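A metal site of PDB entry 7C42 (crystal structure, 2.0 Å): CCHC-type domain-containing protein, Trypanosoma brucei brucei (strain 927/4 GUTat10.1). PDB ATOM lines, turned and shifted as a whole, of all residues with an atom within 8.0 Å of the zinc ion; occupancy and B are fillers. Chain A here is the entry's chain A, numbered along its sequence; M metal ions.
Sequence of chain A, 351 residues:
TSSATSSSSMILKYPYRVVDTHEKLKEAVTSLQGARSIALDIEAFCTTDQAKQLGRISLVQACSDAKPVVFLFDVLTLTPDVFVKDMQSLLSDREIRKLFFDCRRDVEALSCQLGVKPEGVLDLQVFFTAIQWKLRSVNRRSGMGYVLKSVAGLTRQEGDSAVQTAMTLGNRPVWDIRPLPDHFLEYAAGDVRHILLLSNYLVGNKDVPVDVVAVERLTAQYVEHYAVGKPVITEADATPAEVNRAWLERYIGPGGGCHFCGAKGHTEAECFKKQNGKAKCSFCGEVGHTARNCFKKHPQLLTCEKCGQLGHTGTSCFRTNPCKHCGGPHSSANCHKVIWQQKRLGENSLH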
ATOM      1  N   GLY A 257      18.900  17.533  15.361  1.00  0.00           N
ATOM      2  CA  GLY A 257      19.533  17.600  14.056  1.00  0.00           C
ATOM      3  C   GLY A 257      18.809  16.704  13.077  1.00  0.00           C
ATOM      4  O   GLY A 257      17.802  16.081  13.407  1.00  0.00           O
ATOM      5  N   CYS A 258      19.326  16.666  11.858  1.00  0.00           N
ATOM      6  CA  CYS A 258      18.650  15.982  10.767  1.00  0.00           C
ATOM      7  C   CYS A 258      18.727  14.469  10.957  1.00  0.00           C
ATOM      8  O   CYS A 258      19.815  13.900  11.087  1.00  0.00           O
ATOM      9  CB  CYS A 258      19.255  16.381   9.430  1.00  0.00           C
ATOM     10  SG  CYS A 258      18.477  15.559   8.010  1.00  0.00           S
ATOM     11  N   HIS A 259      17.573  13.810  10.980  1.00  0.00           N
ATOM     12  CA  HIS A 259      17.567  12.365  11.166  1.00  0.00           C
ATOM     13  C   HIS A 259      18.061  11.637   9.933  1.00  0.00           C
ATOM     14  O   HIS A 259      18.383  10.447  10.015  1.00  0.00           O
ATOM     15  CB  HIS A 259      16.166  11.872  11.490  1.00  0.00           C
ATOM     16  CG  HIS A 259      15.641  12.377  12.798  1.00  0.00           C
ATOM     17  ND1 HIS A 259      14.378  12.096  13.249  1.00  0.00           N
ATOM     18  CD2 HIS A 259      16.218  13.160  13.740  1.00  0.00           C
ATOM     19  CE1 HIS A 259      14.197  12.674  14.426  1.00  0.00           C
ATOM     20  NE2 HIS A 259      15.291  13.330  14.746  1.00  0.00           N
ATOM     21  N   PHE A 260      18.093  12.314   8.782  1.00  0.00           N
ATOM     22  CA  PHE A 260      18.463  11.640   7.554  1.00  0.00           C
ATOM     23  C   PHE A 260      19.969  11.679   7.288  1.00  0.00           C
ATOM     24  O   PHE A 260      20.558  10.661   6.940  1.00  0.00           O
ATOM     25  CB  PHE A 260      17.714  12.244   6.358  1.00  0.00           C
ATOM     26  CG  PHE A 260      17.942  11.474   5.076  1.00  0.00           C
ATOM     27  CD1 PHE A 260      17.210  10.319   4.811  1.00  0.00           C
ATOM     28  CD2 PHE A 260      18.915  11.880   4.158  1.00  0.00           C
ATOM     29  CE1 PHE A 260      17.424   9.597   3.666  1.00  0.00           C
ATOM     30  CE2 PHE A 260      19.130  11.156   2.988  1.00  0.00           C
ATOM     31  CZ  PHE A 260      18.382  10.012   2.736  1.00  0.00           C
ATOM     32  N   CYS A 261      20.608  12.840   7.461  1.00  0.00           N
ATOM     33  CA  CYS A 261      22.041  12.949   7.236  1.00  0.00           C
ATOM     34  C   CYS A 261      22.860  13.142   8.506  1.00  0.00           C
ATOM     35  O   CYS A 261      24.084  13.013   8.454  1.00  0.00           O
ATOM     36  CB  CYS A 261      22.335  14.081   6.242  1.00  0.00           C
ATOM     37  SG  CYS A 261      22.121  15.767   6.861  1.00  0.00           S
ATOM     38  N   GLY A 262      22.232  13.444   9.643  1.00  0.00           N
ATOM     39  CA  GLY A 262      22.949  13.585  10.889  1.00  0.00           C
ATOM     40  C   GLY A 262      23.418  14.982  11.226  1.00  0.00           C
ATOM     41  O   GLY A 262      23.861  15.213  12.351  1.00  0.00           O
ATOM     42  N   ALA A 263      23.334  15.927  10.282  1.00  0.00           N
ATOM     43  CA  ALA A 263      23.858  17.265  10.507  1.00  0.00           C
ATOM     44  C   ALA A 263      22.949  18.093  11.417  1.00  0.00           C
ATOM     45  O   ALA A 263      21.725  18.009  11.336  1.00  0.00           O
ATOM     46  CB  ALA A 263      24.021  17.996   9.167  1.00  0.00           C
ATOM     47  N   LYS A 264      23.552  18.911  12.284  1.00  0.00           N
ATOM     48  CA  LYS A 264      22.759  19.923  12.970  1.00  0.00           C
ATOM     49  C   LYS A 264      22.389  21.054  12.007  1.00  0.00           C
ATOM     50  O   LYS A 264      22.957  21.193  10.918  1.00  0.00           O
ATOM     51  CB  LYS A 264      23.478  20.454  14.215  1.00  0.00           C
ATOM     52  CG  LYS A 264      24.042  19.327  15.069  1.00  0.00           C
ATOM     53  CD  LYS A 264      25.069  19.746  16.113  1.00  0.00           C
ATOM     54  CE  LYS A 264      24.619  19.325  17.510  1.00  0.00           C
ATOM     55  NZ  LYS A 264      24.478  17.837  17.618  1.00  0.00           N
ATOM     56  N   GLY A 265      21.390  21.819  12.395  1.00  0.00           N
ATOM     57  CA  GLY A 265      20.997  23.002  11.646  1.00  0.00           C
ATOM     58  C   GLY A 265      19.788  22.858  10.755  1.00  0.00           C
ATOM     59  O   GLY A 265      19.261  23.884  10.310  1.00  0.00           O
ATOM     60  N   HIS A 266      19.332  21.642  10.459  1.00  0.00           N
ATOM     61  CA  HIS A 266      18.120  21.494   9.662  1.00  0.00           C
ATOM     62  C   HIS A 266      17.455  20.179  10.015  1.00  0.00           C
ATOM     63  O   HIS A 266      18.038  19.324  10.681  1.00  0.00           O
ATOM     64  CB  HIS A 266      18.388  21.554   8.150  1.00  0.00           C
ATOM     65  CG  HIS A 266      19.146  20.364   7.623  1.00  0.00           C
ATOM     66  ND1 HIS A 266      20.519  20.319   7.568  1.00  0.00           N
ATOM     67  CD2 HIS A 266      18.708  19.179   7.134  1.00  0.00           C
ATOM     68  CE1 HIS A 266      20.897  19.165   7.065  1.00  0.00           C
ATOM     69  NE2 HIS A 266      19.827  18.452   6.790  1.00  0.00           N
ATOM     70  N   THR A 267      16.209  20.040   9.593  1.00  0.00           N
ATOM     71  CA  THR A 267      15.470  18.814   9.806  1.00  0.00           C
ATOM     72  C   THR A 267      15.431  18.005   8.523  1.00  0.00           C
ATOM     73  O   THR A 267      15.800  18.463   7.439  1.00  0.00           O
ATOM     74  CB  THR A 267      14.052  19.097  10.287  1.00  0.00           C
ATOM     75  OG1 THR A 267      13.339  19.791   9.255  1.00  0.00           O
ATOM     76  CG2 THR A 267      14.088  19.947  11.556  1.00  0.00           C
ATOM     77  N   GLU A 268      14.976  16.777   8.661  1.00  0.00           N
ATOM     78  CA  GLU A 268      14.936  15.889   7.517  1.00  0.00           C
ATOM     79  C   GLU A 268      13.984  16.405   6.450  1.00  0.00           C
ATOM     80  O   GLU A 268      14.240  16.248   5.258  1.00  0.00           O
ATOM     81  CB  GLU A 268      14.607  14.495   8.032  1.00  0.00           C
ATOM     82  CG  GLU A 268      13.662  13.722   7.249  1.00  0.00           C
ATOM     83  CD  GLU A 268      13.447  12.380   7.890  1.00  0.00           C
ATOM     84  OE1 GLU A 268      13.561  12.271   9.134  1.00  0.00           O
ATOM     85  OE2 GLU A 268      13.222  11.423   7.139  1.00  0.00           O
ATOM     86  N   ALA A 269      12.904  17.078   6.846  1.00  0.00           N
ATOM     87  CA  ALA A 269      12.022  17.706   5.869  1.00  0.00           C
ATOM     88  C   ALA A 269      12.746  18.775   5.046  1.00  0.00           C
ATOM     89  O   ALA A 269      12.324  19.054   3.913  1.00  0.00           O
ATOM     90  CB  ALA A 269      10.808  18.333   6.544  1.00  0.00           C
ATOM     91  N   GLU A 270      13.807  19.362   5.580  1.00  0.00           N
ATOM     92  CA  GLU A 270      14.556  20.400   4.873  1.00  0.00           C
ATOM     93  C   GLU A 270      15.819  19.863   4.215  1.00  0.00           C
ATOM     94  O   GLU A 270      16.587  20.646   3.655  1.00  0.00           O
ATOM     95  CB  GLU A 270      14.935  21.539   5.838  1.00  0.00           C
ATOM     96  CG  GLU A 270      13.792  22.010   6.737  1.00  0.00           C
ATOM     97  CD  GLU A 270      14.258  22.813   7.947  1.00  0.00           C
ATOM     98  OE1 GLU A 270      15.270  22.431   8.595  1.00  0.00           O
ATOM     99  OE2 GLU A 270      13.612  23.825   8.266  1.00  0.00           O
ATOM    100  N   CYS A 271      16.059  18.557   4.282  1.00  0.00           N
ATOM    101  CA  CYS A 271      17.357  18.006   3.935  1.00  0.00           C
ATOM    102  C   CYS A 271      17.525  17.939   2.419  1.00  0.00           C
ATOM    103  O   CYS A 271      16.748  17.275   1.723  1.00  0.00           O
ATOM    104  CB  CYS A 271      17.522  16.627   4.552  1.00  0.00           C
ATOM    105  SG  CYS A 271      19.152  15.941   4.317  1.00  0.00           S
ATOM    106  N   PHE A 272      18.531  18.630   1.898  1.00  0.00           N
ATOM    107  CA  PHE A 272      18.786  18.528   0.462  1.00  0.00           C
ATOM    108  C   PHE A 272      19.237  17.128   0.077  1.00  0.00           C
ATOM    109  O   PHE A 272      18.824  16.612  -0.969  1.00  0.00           O
ATOM    110  CB  PHE A 272      19.817  19.567   0.027  1.00  0.00           C
ATOM    111  CG  PHE A 272      20.081  19.548  -1.453  1.00  0.00           C
ATOM    112  CD1 PHE A 272      19.132  20.018  -2.354  1.00  0.00           C
ATOM    113  CD2 PHE A 272      21.276  19.029  -1.945  1.00  0.00           C
ATOM    114  CE1 PHE A 272      19.381  19.988  -3.715  1.00  0.00           C
ATOM    115  CE2 PHE A 272      21.525  18.999  -3.306  1.00  0.00           C
ATOM    116  CZ  PHE A 272      20.572  19.475  -4.191  1.00  0.00           C
ATOM    117  N   LYS A 273      20.082  16.509   0.894  1.00  0.00           N
ATOM    118  CA  LYS A 273      20.567  15.173   0.576  1.00  0.00           C
ATOM    119  C   LYS A 273      19.407  14.176   0.452  1.00  0.00           C
ATOM    120  O   LYS A 273      19.418  13.309  -0.427  1.00  0.00           O
ATOM    121  CB  LYS A 273      21.562  14.693   1.634  1.00  0.00           C
ATOM    122  CG  LYS A 273      22.881  15.463   1.639  1.00  0.00           C
ATOM    123  CD  LYS A 273      23.836  14.854   2.657  1.00  0.00           C
ATOM    124  CE  LYS A 273      25.126  15.630   2.772  1.00  0.00           C
ATOM    125  NZ  LYS A 273      26.008  15.028   3.821  1.00  0.00           N
ATOM    126  N   LYS A 274      18.395  14.313   1.319  1.00  0.00           N
ATOM    127  CA  LYS A 274      17.253  13.403   1.245  1.00  0.00           C
ATOM    128  C   LYS A 274      16.510  13.566  -0.074  1.00  0.00           C
ATOM    129  O   LYS A 274      16.274  12.589  -0.795  1.00  0.00           O
ATOM    130  CB  LYS A 274      16.313  13.622   2.436  1.00  0.00           C
ATOM    131  CG  LYS A 274      15.172  12.625   2.434  1.00  0.00           C
ATOM    132  CD  LYS A 274      14.377  12.654   3.721  1.00  0.00           C
ATOM    133  CE  LYS A 274      13.377  11.494   3.700  1.00  0.00           C
ATOM    134  NZ  LYS A 274      12.338  11.628   4.755  1.00  0.00           N
HETATM  135 ZN    ZN M   1      20.060  16.368   6.422  1.00  0.00          ZN
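The side-chain sulfur (SG) of Cys 261 lies close to the backbone NH (N) of Ala 263 (3.6 Å). The side-chain sulfur of Cys 271 sits close to the backbone NH of Lys 273, at 3.6 Å. SG of Cys 271 lies close to N of Lys 274, 3.5 Å away. The backbone NH (N) of Phe 260 lies close to the side-chain sulfur (SG) of Cys 258. The backbone carbonyl oxygen (O) of Ala 263 is in hydrogen-bond range of the backbone NH (N) of Cys 258, 2.8 Å away. N of Glu 268 sits close to SG of Cys 258, at 3.8 Å.
Of the 18 residues printed, 4 come within 4 Å of the zinc ion.
The zinc ion is bound by a ring nitrogen (NE2) of His 266 (2.1 Å), the side-chain sulfur (SG) of Cys 261 (2.2 Å), the side-chain sulfur (SG) of Cys 271 (2.3 Å) and the side-chain sulfur (SG) of Cys 258 (2.4 Å).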
